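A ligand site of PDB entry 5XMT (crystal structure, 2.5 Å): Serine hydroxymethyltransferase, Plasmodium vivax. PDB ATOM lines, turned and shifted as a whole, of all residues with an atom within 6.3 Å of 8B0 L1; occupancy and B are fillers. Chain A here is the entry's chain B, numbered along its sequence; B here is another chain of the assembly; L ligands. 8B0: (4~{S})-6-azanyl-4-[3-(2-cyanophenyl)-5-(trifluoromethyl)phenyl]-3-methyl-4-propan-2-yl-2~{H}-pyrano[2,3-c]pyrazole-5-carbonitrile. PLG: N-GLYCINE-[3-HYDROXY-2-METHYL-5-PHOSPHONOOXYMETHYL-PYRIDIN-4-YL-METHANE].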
ATOM      1  N   HIS A 123     -28.749  15.759  -2.986  1.00  0.00           N
ATOM      2  CA  HIS A 123     -27.589  16.065  -3.826  1.00  0.00           C
ATOM      3  C   HIS A 123     -27.848  15.549  -5.243  1.00  0.00           C
ATOM      4  O   HIS A 123     -28.488  14.493  -5.433  1.00  0.00           O
ATOM      5  CB  HIS A 123     -26.332  15.396  -3.272  1.00  0.00           C
ATOM      6  CG  HIS A 123     -25.068  16.116  -3.597  1.00  0.00           C
ATOM      7  ND1 HIS A 123     -24.335  15.877  -4.733  1.00  0.00           N
ATOM      8  CD2 HIS A 123     -24.356  17.033  -2.895  1.00  0.00           C
ATOM      9  CE1 HIS A 123     -23.250  16.636  -4.749  1.00  0.00           C
ATOM     10  NE2 HIS A 123     -23.245  17.351  -3.646  1.00  0.00           N
ATOM     11  N   LEU A 124     -27.362  16.290  -6.235  1.00  0.00           N
ATOM     12  CA  LEU A 124     -27.493  15.912  -7.648  1.00  0.00           C
ATOM     13  C   LEU A 124     -26.914  14.513  -7.892  1.00  0.00           C
ATOM     14  O   LEU A 124     -27.543  13.677  -8.554  1.00  0.00           O
ATOM     15  CB  LEU A 124     -26.787  16.924  -8.539  1.00  0.00           C
ATOM     16  CG  LEU A 124     -26.897  16.816 -10.052  1.00  0.00           C
ATOM     17  CD1 LEU A 124     -28.159  17.478 -10.553  1.00  0.00           C
ATOM     18  CD2 LEU A 124     -25.689  17.475 -10.705  1.00  0.00           C
ATOM     19  N   CYS A 125     -25.715  14.299  -7.358  1.00  0.00           N
ATOM     20  CA  CYS A 125     -25.013  13.014  -7.456  1.00  0.00           C
ATOM     21  C   CYS A 125     -25.735  11.828  -6.764  1.00  0.00           C
ATOM     22  O   CYS A 125     -25.564  10.693  -7.166  1.00  0.00           O
ATOM     23  CB  CYS A 125     -23.560  13.145  -6.967  1.00  0.00           C
ATOM     24  SG  CYS A 125     -22.565  14.495  -7.712  1.00  0.00           S
ATOM     25  N   SER A 126     -26.559  12.100  -5.754  1.00  0.00           N
ATOM     26  CA  SER A 126     -27.363  11.081  -5.114  1.00  0.00           C
ATOM     27  C   SER A 126     -28.713  10.911  -5.798  1.00  0.00           C
ATOM     28  O   SER A 126     -29.449   9.986  -5.455  1.00  0.00           O
ATOM     29  CB  SER A 126     -27.602  11.421  -3.633  1.00  0.00           C
ATOM     30  OG  SER A 126     -26.371  11.543  -2.916  1.00  0.00           O
ATOM     31  N   GLY A 127     -29.067  11.800  -6.713  1.00  0.00           N
ATOM     32  CA  GLY A 127     -30.281  11.638  -7.512  1.00  0.00           C
ATOM     33  C   GLY A 127     -31.315  12.734  -7.416  1.00  0.00           C
ATOM     34  O   GLY A 127     -32.400  12.577  -7.964  1.00  0.00           O
ATOM     35  N   GLY A 128     -30.994  13.848  -6.749  1.00  0.00           N
ATOM     36  CA  GLY A 128     -31.862  15.001  -6.740  1.00  0.00           C
ATOM     37  C   GLY A 128     -31.664  15.849  -7.988  1.00  0.00           C
ATOM     38  O   GLY A 128     -30.751  15.609  -8.766  1.00  0.00           O
ATOM     39  N   HIS A 129     -32.561  16.801  -8.182  1.00  0.00           N
ATOM     40  CA  HIS A 129     -32.475  17.711  -9.294  1.00  0.00           C
ATOM     41  C   HIS A 129     -31.581  18.884  -9.008  1.00  0.00           C
ATOM     42  O   HIS A 129     -31.268  19.183  -7.860  1.00  0.00           O
ATOM     43  CB  HIS A 129     -33.866  18.186  -9.710  1.00  0.00           C
ATOM     44  CG  HIS A 129     -33.902  18.722 -11.110  1.00  0.00           C
ATOM     45  ND1 HIS A 129     -34.120  20.050 -11.392  1.00  0.00           N
ATOM     46  CD2 HIS A 129     -33.641  18.118 -12.293  1.00  0.00           C
ATOM     47  CE1 HIS A 129     -34.030  20.239 -12.697  1.00  0.00           C
ATOM     48  NE2 HIS A 129     -33.760  19.086 -13.259  1.00  0.00           N
ATOM     49  N   LEU A 130     -31.141  19.504 -10.101  1.00  0.00           N
ATOM     50  CA  LEU A 130     -30.390  20.753 -10.070  1.00  0.00           C
ATOM     51  C   LEU A 130     -31.112  21.828  -9.275  1.00  0.00           C
ATOM     52  O   LEU A 130     -30.495  22.522  -8.457  1.00  0.00           O
ATOM     53  CB  LEU A 130     -30.153  21.241 -11.503  1.00  0.00           C
ATOM     54  CG  LEU A 130     -29.155  20.402 -12.301  1.00  0.00           C
ATOM     55  CD1 LEU A 130     -29.492  20.439 -13.788  1.00  0.00           C
ATOM     56  CD2 LEU A 130     -27.720  20.873 -12.038  1.00  0.00           C
ATOM     57  N   PHE A 134     -28.656  22.378  -5.804  1.00  0.00           N
ATOM     58  CA  PHE A 134     -27.376  21.822  -6.159  1.00  0.00           C
ATOM     59  C   PHE A 134     -26.286  22.884  -6.223  1.00  0.00           C
ATOM     60  O   PHE A 134     -26.452  23.907  -6.883  1.00  0.00           O
ATOM     61  CB  PHE A 134     -27.408  21.111  -7.514  1.00  0.00           C
ATOM     62  CG  PHE A 134     -26.062  20.606  -7.913  1.00  0.00           C
ATOM     63  CD1 PHE A 134     -25.422  19.634  -7.124  1.00  0.00           C
ATOM     64  CD2 PHE A 134     -25.391  21.152  -8.980  1.00  0.00           C
ATOM     65  CE1 PHE A 134     -24.149  19.184  -7.447  1.00  0.00           C
ATOM     66  CE2 PHE A 134     -24.120  20.708  -9.315  1.00  0.00           C
ATOM     67  CZ  PHE A 134     -23.499  19.725  -8.544  1.00  0.00           C
ATOM     68  N   ASP A 136     -21.562  23.193  -5.914  1.00  0.00           N
ATOM     69  CA  ASP A 136     -20.241  22.602  -5.955  1.00  0.00           C
ATOM     70  C   ASP A 136     -19.335  23.465  -5.087  1.00  0.00           C
ATOM     71  O   ASP A 136     -19.607  24.652  -4.880  1.00  0.00           O
ATOM     72  CB  ASP A 136     -19.747  22.619  -7.411  1.00  0.00           C
ATOM     73  CG  ASP A 136     -18.972  21.374  -7.811  1.00  0.00           C
ATOM     74  OD1 ASP A 136     -19.358  20.262  -7.396  1.00  0.00           O
ATOM     75  OD2 ASP A 136     -17.975  21.505  -8.561  1.00  0.00           O
ATOM     76  N   VAL A 141     -23.995  26.318  -8.540  1.00  0.00           N
ATOM     77  CA  VAL A 141     -24.269  25.863  -9.923  1.00  0.00           C
ATOM     78  C   VAL A 141     -25.710  26.188 -10.317  1.00  0.00           C
ATOM     79  O   VAL A 141     -25.954  26.691 -11.398  1.00  0.00           O
ATOM     80  CB  VAL A 141     -24.001  24.333 -10.071  1.00  0.00           C
ATOM     81  CG1 VAL A 141     -24.104  23.886 -11.526  1.00  0.00           C
ATOM     82  CG2 VAL A 141     -22.620  23.959  -9.528  1.00  0.00           C
ATOM     83  N   THR A 183     -34.885  12.934  -9.367  1.00  0.00           N
ATOM     84  CA  THR A 183     -34.658  12.829 -10.812  1.00  0.00           C
ATOM     85  C   THR A 183     -34.201  11.422 -11.212  1.00  0.00           C
ATOM     86  O   THR A 183     -34.643  10.944 -12.247  1.00  0.00           O
ATOM     87  CB  THR A 183     -33.784  13.978 -11.417  1.00  0.00           C
ATOM     88  OG1 THR A 183     -32.765  13.422 -12.267  1.00  0.00           O
ATOM     89  CG2 THR A 183     -33.175  14.783 -10.403  1.00  0.00           C
ATOM     90  N   SER A 184     -33.385  10.753 -10.394  1.00  0.00           N
ATOM     91  CA  SER A 184     -33.000   9.342 -10.628  1.00  0.00           C
ATOM     92  C   SER A 184     -33.078   8.511  -9.372  1.00  0.00           C
ATOM     93  O   SER A 184     -32.075   8.073  -8.838  1.00  0.00           O
ATOM     94  CB  SER A 184     -31.604   9.196 -11.257  1.00  0.00           C
ATOM     95  OG  SER A 184     -30.860  10.399 -11.224  1.00  0.00           O
ATOM     96  N   GLN A 343     -22.718   4.771 -22.488  1.00  0.00           N
ATOM     97  CA  GLN A 343     -23.546   5.759 -23.213  1.00  0.00           C
ATOM     98  C   GLN A 343     -23.087   5.864 -24.664  1.00  0.00           C
ATOM     99  O   GLN A 343     -23.889   5.796 -25.597  1.00  0.00           O
ATOM    100  CB  GLN A 343     -23.498   7.141 -22.535  1.00  0.00           C
ATOM    101  CG  GLN A 343     -24.774   7.975 -22.670  1.00  0.00           C
ATOM    102  CD  GLN A 343     -24.636   9.332 -21.983  1.00  0.00           C
ATOM    103  OE1 GLN A 343     -24.980   9.489 -20.826  1.00  0.00           O
ATOM    104  NE2 GLN A 343     -24.131  10.326 -22.695  1.00  0.00           N
ATOM    105  N   ASN A 354     -28.546   7.241 -20.291  1.00  0.00           N
ATOM    106  CA  ASN A 354     -27.606   8.225 -19.813  1.00  0.00           C
ATOM    107  C   ASN A 354     -26.820   7.706 -18.644  1.00  0.00           C
ATOM    108  O   ASN A 354     -27.249   6.804 -17.958  1.00  0.00           O
ATOM    109  CB  ASN A 354     -28.286   9.564 -19.450  1.00  0.00           C
ATOM    110  CG  ASN A 354     -29.202   9.473 -18.251  1.00  0.00           C
ATOM    111  OD1 ASN A 354     -30.369   9.117 -18.365  1.00  0.00           O
ATOM    112  ND2 ASN A 354     -28.661   9.782 -17.081  1.00  0.00           N
ATOM    113  N   LYS A 355     -25.667   8.308 -18.457  1.00  0.00           N
ATOM    114  CA  LYS A 355     -24.822   8.020 -17.303  1.00  0.00           C
ATOM    115  C   LYS A 355     -25.463   8.586 -16.042  1.00  0.00           C
ATOM    116  O   LYS A 355     -26.157   9.592 -16.081  1.00  0.00           O
ATOM    117  CB  LYS A 355     -23.383   8.569 -17.438  1.00  0.00           C
ATOM    118  CG  LYS A 355     -23.252   9.821 -18.285  1.00  0.00           C
ATOM    119  CD  LYS A 355     -22.021  10.649 -18.006  1.00  0.00           C
ATOM    120  CE  LYS A 355     -22.124  11.921 -18.843  1.00  0.00           C
ATOM    121  NZ  LYS A 355     -20.797  12.455 -19.164  1.00  0.00           N
ATOM    122  N   ASN A 356     -25.176   7.936 -14.948  1.00  0.00           N
ATOM    123  CA  ASN A 356     -25.790   8.226 -13.690  1.00  0.00           C
ATOM    124  C   ASN A 356     -24.835   7.788 -12.604  1.00  0.00           C
ATOM    125  O   ASN A 356     -24.222   6.709 -12.691  1.00  0.00           O
ATOM    126  CB  ASN A 356     -27.119   7.467 -13.573  1.00  0.00           C
ATOM    127  CG  ASN A 356     -28.095   8.149 -12.635  1.00  0.00           C
ATOM    128  OD1 ASN A 356     -28.147   7.832 -11.469  1.00  0.00           O
ATOM    129  ND2 ASN A 356     -28.838   9.106 -13.151  1.00  0.00           N
ATOM    130  N   THR A 357     -24.739   8.607 -11.572  1.00  0.00           N
ATOM    131  CA  THR A 357     -23.905   8.285 -10.408  1.00  0.00           C
ATOM    132  C   THR A 357     -24.446   7.102  -9.641  1.00  0.00           C
ATOM    133  O   THR A 357     -25.609   6.714  -9.829  1.00  0.00           O
ATOM    134  CB  THR A 357     -23.817   9.477  -9.465  1.00  0.00           C
ATOM    135  OG1 THR A 357     -25.147  10.019  -9.285  1.00  0.00           O
ATOM    136  CG2 THR A 357     -22.908  10.540 -10.065  1.00  0.00           C
ATOM    137  N   CYS A 364     -19.844  13.538  -9.121  1.00  0.00           N
ATOM    138  CA  CYS A 364     -20.421  13.426 -10.465  1.00  0.00           C
ATOM    139  C   CYS A 364     -19.331  13.435 -11.605  1.00  0.00           C
ATOM    140  O   CYS A 364     -19.662  13.629 -12.794  1.00  0.00           O
ATOM    141  CB  CYS A 364     -21.457  14.570 -10.676  1.00  0.00           C
ATOM    142  SG  CYS A 364     -23.035  14.553  -9.720  1.00  0.00           S
ATOM    143  N   VAL A 365     -18.061  13.188 -11.248  1.00  0.00           N
ATOM    144  CA  VAL A 365     -16.914  13.300 -12.177  1.00  0.00           C
ATOM    145  C   VAL A 365     -16.819  12.088 -13.121  1.00  0.00           C
ATOM    146  O   VAL A 365     -16.728  12.257 -14.348  1.00  0.00           O
ATOM    147  CB  VAL A 365     -15.572  13.484 -11.404  1.00  0.00           C
ATOM    148  CG1 VAL A 365     -14.356  13.388 -12.333  1.00  0.00           C
ATOM    149  CG2 VAL A 365     -15.562  14.826 -10.674  1.00  0.00           C
ATOM    150  N   PRO A 367     -19.173   8.929 -13.295  1.00  0.00           N
ATOM    151  CA  PRO A 367     -20.301   8.131 -12.820  1.00  0.00           C
ATOM    152  C   PRO A 367     -20.204   6.690 -13.299  1.00  0.00           C
ATOM    153  O   PRO A 367     -19.925   6.463 -14.479  1.00  0.00           O
ATOM    154  CB  PRO A 367     -21.508   8.828 -13.444  1.00  0.00           C
ATOM    155  CG  PRO A 367     -20.972   9.445 -14.680  1.00  0.00           C
ATOM    156  CD  PRO A 367     -19.603   9.922 -14.295  1.00  0.00           C
ATOM    157  N   ARG A 371     -28.682   5.095 -16.229  1.00  0.00           N
ATOM    158  CA  ARG A 371     -30.064   5.132 -15.869  1.00  0.00           C
ATOM    159  C   ARG A 371     -30.922   4.866 -17.078  1.00  0.00           C
ATOM    160  O   ARG A 371     -30.737   5.479 -18.121  1.00  0.00           O
ATOM    161  CB  ARG A 371     -30.425   6.499 -15.299  1.00  0.00           C
ATOM    162  CG  ARG A 371     -31.899   6.635 -14.949  1.00  0.00           C
ATOM    163  CD  ARG A 371     -32.230   8.063 -14.605  1.00  0.00           C
ATOM    164  NE  ARG A 371     -32.296   8.906 -15.784  1.00  0.00           N
ATOM    165  CZ  ARG A 371     -32.832  10.128 -15.810  1.00  0.00           C
ATOM    166  NH1 ARG A 371     -33.378  10.651 -14.713  1.00  0.00           N
ATOM    167  NH2 ARG A 371     -32.828  10.841 -16.949  1.00  0.00           N
ATOM    168  N   GLU B  56     -30.331  18.928 -22.514  1.00  0.00           N
ATOM    169  CA  GLU B  56     -29.670  19.821 -21.587  1.00  0.00           C
ATOM    170  C   GLU B  56     -28.221  20.019 -21.994  1.00  0.00           C
ATOM    171  O   GLU B  56     -27.515  19.065 -22.335  1.00  0.00           O
ATOM    172  CB  GLU B  56     -29.734  19.234 -20.184  1.00  0.00           C
ATOM    173  CG  GLU B  56     -31.127  19.252 -19.589  1.00  0.00           C
ATOM    174  CD  GLU B  56     -31.201  18.444 -18.330  1.00  0.00           C
ATOM    175  OE1 GLU B  56     -31.589  17.263 -18.395  1.00  0.00           O
ATOM    176  OE2 GLU B  56     -30.847  18.982 -17.263  1.00  0.00           O
ATOM    177  N   TYR B  63     -25.288  16.639 -22.235  1.00  0.00           N
ATOM    178  CA  TYR B  63     -25.291  15.548 -21.266  1.00  0.00           C
ATOM    179  C   TYR B  63     -25.708  14.229 -21.906  1.00  0.00           C
ATOM    180  O   TYR B  63     -25.137  13.217 -21.544  1.00  0.00           O
ATOM    181  CB  TYR B  63     -26.124  15.909 -20.022  1.00  0.00           C
ATOM    182  CG  TYR B  63     -25.318  16.832 -19.143  1.00  0.00           C
ATOM    183  CD1 TYR B  63     -24.353  16.307 -18.282  1.00  0.00           C
ATOM    184  CD2 TYR B  63     -25.423  18.207 -19.238  1.00  0.00           C
ATOM    185  CE1 TYR B  63     -23.547  17.135 -17.500  1.00  0.00           C
ATOM    186  CE2 TYR B  63     -24.630  19.038 -18.468  1.00  0.00           C
ATOM    187  CZ  TYR B  63     -23.690  18.499 -17.592  1.00  0.00           C
ATOM    188  OH  TYR B  63     -22.885  19.324 -16.820  1.00  0.00           O
ATOM    189  N   TYR B  64     -26.666  14.238 -22.823  1.00  0.00           N
ATOM    190  CA  TYR B  64     -27.130  13.005 -23.490  1.00  0.00           C
ATOM    191  C   TYR B  64     -26.670  12.959 -24.938  1.00  0.00           C
ATOM    192  O   TYR B  64     -26.401  13.994 -25.562  1.00  0.00           O
ATOM    193  CB  TYR B  64     -28.652  12.863 -23.476  1.00  0.00           C
ATOM    194  CG  TYR B  64     -29.344  12.973 -22.124  1.00  0.00           C
ATOM    195  CD1 TYR B  64     -28.638  13.035 -20.930  1.00  0.00           C
ATOM    196  CD2 TYR B  64     -30.748  12.982 -22.048  1.00  0.00           C
ATOM    197  CE1 TYR B  64     -29.283  13.125 -19.727  1.00  0.00           C
ATOM    198  CE2 TYR B  64     -31.403  13.076 -20.826  1.00  0.00           C
ATOM    199  CZ  TYR B  64     -30.661  13.150 -19.666  1.00  0.00           C
ATOM    200  OH  TYR B  64     -31.265  13.247 -18.444  1.00  0.00           O
ATOM    201  N   PHE B 266     -28.477  27.775 -18.512  1.00  0.00           N
ATOM    202  CA  PHE B 266     -28.377  26.401 -18.011  1.00  0.00           C
ATOM    203  C   PHE B 266     -26.976  26.138 -17.480  1.00  0.00           C
ATOM    204  O   PHE B 266     -26.023  26.397 -18.195  1.00  0.00           O
ATOM    205  CB  PHE B 266     -28.676  25.404 -19.109  1.00  0.00           C
ATOM    206  CG  PHE B 266     -28.515  23.984 -18.676  1.00  0.00           C
ATOM    207  CD1 PHE B 266     -29.534  23.327 -17.990  1.00  0.00           C
ATOM    208  CD2 PHE B 266     -27.332  23.281 -18.916  1.00  0.00           C
ATOM    209  CE1 PHE B 266     -29.392  22.005 -17.576  1.00  0.00           C
ATOM    210  CE2 PHE B 266     -27.180  21.962 -18.502  1.00  0.00           C
ATOM    211  CZ  PHE B 266     -28.204  21.320 -17.831  1.00  0.00           C
ATOM    212  N   PRO B 267     -26.815  25.593 -16.273  1.00  0.00           N
ATOM    213  CA  PRO B 267     -27.895  25.040 -15.431  1.00  0.00           C
ATOM    214  C   PRO B 267     -28.391  25.942 -14.319  1.00  0.00           C
ATOM    215  O   PRO B 267     -29.037  25.459 -13.396  1.00  0.00           O
ATOM    216  CB  PRO B 267     -27.183  23.858 -14.766  1.00  0.00           C
ATOM    217  CG  PRO B 267     -25.827  24.434 -14.473  1.00  0.00           C
ATOM    218  CD  PRO B 267     -25.497  25.221 -15.732  1.00  0.00           C
HETATM  219  C2  8B0 L   1     -29.363  14.332 -11.878  1.00  0.00           C
HETATM  220  C3  8B0 L   1     -28.339  13.887 -12.656  1.00  0.00           C
HETATM  221  C4  8B0 L   1     -28.091  14.369 -14.087  1.00  0.00           C
HETATM  222  C5  8B0 L   1     -29.045  15.486 -14.434  1.00  0.00           C
HETATM  223  C6  8B0 L   1     -30.141  15.917 -13.560  1.00  0.00           C
HETATM  224  C10 8B0 L   1     -29.236  16.403 -15.605  1.00  0.00           C
HETATM  225  C12 8B0 L   1     -28.458  16.524 -16.889  1.00  0.00           C
HETATM  226  C13 8B0 L   1     -28.404  13.169 -15.010  1.00  0.00           C
HETATM  227  C14 8B0 L   1     -27.924  13.346 -16.462  1.00  0.00           C
HETATM  228  C15 8B0 L   1     -26.625  14.871 -14.187  1.00  0.00           C
HETATM  229  C16 8B0 L   1     -25.563  13.978 -14.394  1.00  0.00           C
HETATM  230  C17 8B0 L   1     -24.224  14.372 -14.506  1.00  0.00           C
HETATM  231  C19 8B0 L   1     -24.932  16.651 -14.170  1.00  0.00           C
HETATM  232  N53 8B0 L   1     -22.294  17.307 -11.760  1.00  0.00           N
HETATM  233  C50 8B0 L   1     -22.937  17.942 -12.471  1.00  0.00           C
HETATM  234  C39 8B0 L   1     -23.646  18.646 -13.245  1.00  0.00           C
HETATM  235  C40 8B0 L   1     -23.394  20.007 -13.204  1.00  0.00           C
HETATM  236  C41 8B0 L   1     -24.116  20.861 -14.012  1.00  0.00           C
HETATM  237  C42 8B0 L   1     -25.107  20.339 -14.856  1.00  0.00           C
HETATM  238  C43 8B0 L   1     -25.356  18.969 -14.894  1.00  0.00           C
HETATM  239  C32 8B0 L   1     -24.621  18.109 -14.084  1.00  0.00           C
HETATM  240  C18 8B0 L   1     -23.924  15.727 -14.390  1.00  0.00           C
HETATM  241  C33 8B0 L   1     -23.173  13.294 -14.742  1.00  0.00           C
HETATM  242  F48 8B0 L   1     -21.941  13.767 -14.880  1.00  0.00           F
HETATM  243  F47 8B0 L   1     -23.484  12.601 -15.826  1.00  0.00           F
HETATM  244  F46 8B0 L   1     -23.178  12.444 -13.730  1.00  0.00           F
HETATM  245  C20 8B0 L   1     -26.274  16.230 -14.071  1.00  0.00           C
HETATM  246  C34 8B0 L   1     -29.881  12.719 -15.019  1.00  0.00           C
HETATM  247  C8  8B0 L   1     -27.561  13.008 -12.204  1.00  0.00           C
HETATM  248  N9  8B0 L   1     -26.843  12.190 -11.783  1.00  0.00           N
HETATM  249  N7  8B0 L   1     -29.586  13.898 -10.638  1.00  0.00           N
HETATM  250  N51 8B0 L   1     -30.302  17.185 -15.293  1.00  0.00           N
HETATM  251  N11 8B0 L   1     -30.889  16.934 -14.051  1.00  0.00           N
HETATM  252  O1  8B0 L   1     -30.321  15.323 -12.355  1.00  0.00           O
HETATM  253  N1  PLG L   2     -37.756  18.225 -11.368  1.00  0.00           N
HETATM  254  C2  PLG L   2     -37.298  16.957 -11.454  1.00  0.00           C
HETATM  255  C2A PLG L   2     -37.472  16.001 -10.299  1.00  0.00           C
HETATM  256  C3  PLG L   2     -36.634  16.535 -12.694  1.00  0.00           C
HETATM  257  O3  PLG L   2     -36.183  15.280 -12.837  1.00  0.00           O
HETATM  258  C4  PLG L   2     -36.496  17.521 -13.786  1.00  0.00           C
HETATM  259  C4A PLG L   2     -35.821  17.190 -15.094  1.00  0.00           C
HETATM  260  C5  PLG L   2     -37.053  18.879 -13.551  1.00  0.00           C
HETATM  261  C6  PLG L   2     -37.655  19.154 -12.319  1.00  0.00           C
HETATM  262  C5A PLG L   2     -36.922  20.018 -14.563  1.00  0.00           C
HETATM  263  OP4 PLG L   2     -37.513  19.826 -15.831  1.00  0.00           O
HETATM  264  P   PLG L   2     -37.158  20.873 -17.010  1.00  0.00           P
HETATM  265  OP1 PLG L   2     -35.933  20.223 -17.660  1.00  0.00           O
HETATM  266  OP2 PLG L   2     -36.835  22.210 -16.470  1.00  0.00           O
HETATM  267  OP3 PLG L   2     -38.470  20.773 -17.755  1.00  0.00           O
HETATM  268  C   PLG L   2     -34.001  14.242 -16.463  1.00  0.00           C
HETATM  269  O   PLG L   2     -34.530  13.378 -15.728  1.00  0.00           O
HETATM  270  OXT PLG L   2     -33.456  13.914 -17.524  1.00  0.00           O
HETATM  271  CA  PLG L   2     -34.035  15.704 -16.051  1.00  0.00           C
HETATM  272  N   PLG L   2     -35.158  15.903 -15.161  1.00  0.00           N
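The guanidinium group (NH1) of Arg 371 is in salt-bridge range of an oxygen (O) of PLG L2 (3.1 Å).
A nitrogen (N51) of 8B0 L1 is in hydrogen-bond range of the side-chain carboxylate of Glu 56 of chain B (2.7 Å).
O of Leu 124 sits at hydrogen-bond distance from N7 of 8B0 L1, at 2.9 Å.
OH of Tyr 64 of chain B is in hydrogen-bond range of OXT of PLG L2, at 2.5 Å.
The backbone carbonyl oxygen of Gly 128 lies within hydrogen-bond range of a nitrogen (N7) of 8B0 L1.
The side-chain hydroxyl (OG1) of Thr 183 is in hydrogen-bond range of an oxygen (O1) of 8B0 L1.
The backbone carbonyl oxygen (O) of Cys 364 lies close to a fluorine (F48) of 8B0 L1 (3.1 Å).
Gly 127 touches 8B0 L1 (C to N7, 3.8 Å).
His 129 touches 8B0 L1 (CD2 to N11, 3.5 Å).
Leu 130 touches 8B0 L1 (CD1 to N51, 3.7 Å).
CG1 of Val 141 touches C41 of 8B0 L1, at 3.9 Å.
OG of Ser 184 touches N7 of 8B0 L1 (3.8 Å).
ND2 of Asn 354 touches C14 of 8B0 L1, 3.7 Å away.
Lys 355 touches 8B0 L1 (CD to F47, 3.3 Å).
ND2 of Asn 356 touches N9 of 8B0 L1, 3.9 Å away.
Thr 357 touches 8B0 L1.
Pro 367 touches 8B0 L1.
Arg 371 touches 8B0 L1 (NH2 to C34, 3.99 Å).
Tyr 63 of chain B touches 8B0 L1.
Tyr 64 of chain B touches 8B0 L1 (CE1 to C14, 3.5 Å).
Pro 267 of chain B touches 8B0 L1.
Hydrophobic or aromatic side chains that line 8B0 L1: Leu 124, His 129, Leu 130, Val 141, Pro 367, Tyr 63 of chain B, Tyr 64 of chain B and Pro 267 of chain B.
Of the 27 residues printed, 19 come within 4 Å of 8B0 L1.
The backbone NH (N) of Tyr 63 of chain B sits at hydrogen-bond distance from the backbone carbonyl oxygen (O) of Glu 56 of chain B (3.3 Å).
N of Thr 183 is in hydrogen-bond range of O of Gly 127, 2.9 Å away.
The backbone NH (N) of Gly 128 lies within hydrogen-bond range of the backbone carbonyl oxygen (O) of His 123 (2.9 Å).
The guanidinium group (NH1) of Arg 371 lies within hydrogen-bond range of the backbone carbonyl oxygen (O) of Thr 183 (2.8 Å).
O of Tyr 63 of chain B lies within hydrogen-bond range of NE2 of Gln 343 (3.3 Å).
The backbone NH (N) of Ser 184 is in hydrogen-bond range of the backbone carbonyl oxygen (O) of Gly 127 (3.2 Å).
SG of Cys 125 is disulfide-bonded to SG of Cys 364 (2.1 Å).
The backbone NH (N) of Arg 371 is in hydrogen-bond range of the backbone carbonyl oxygen (O) of Asn 354 (2.8 Å).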
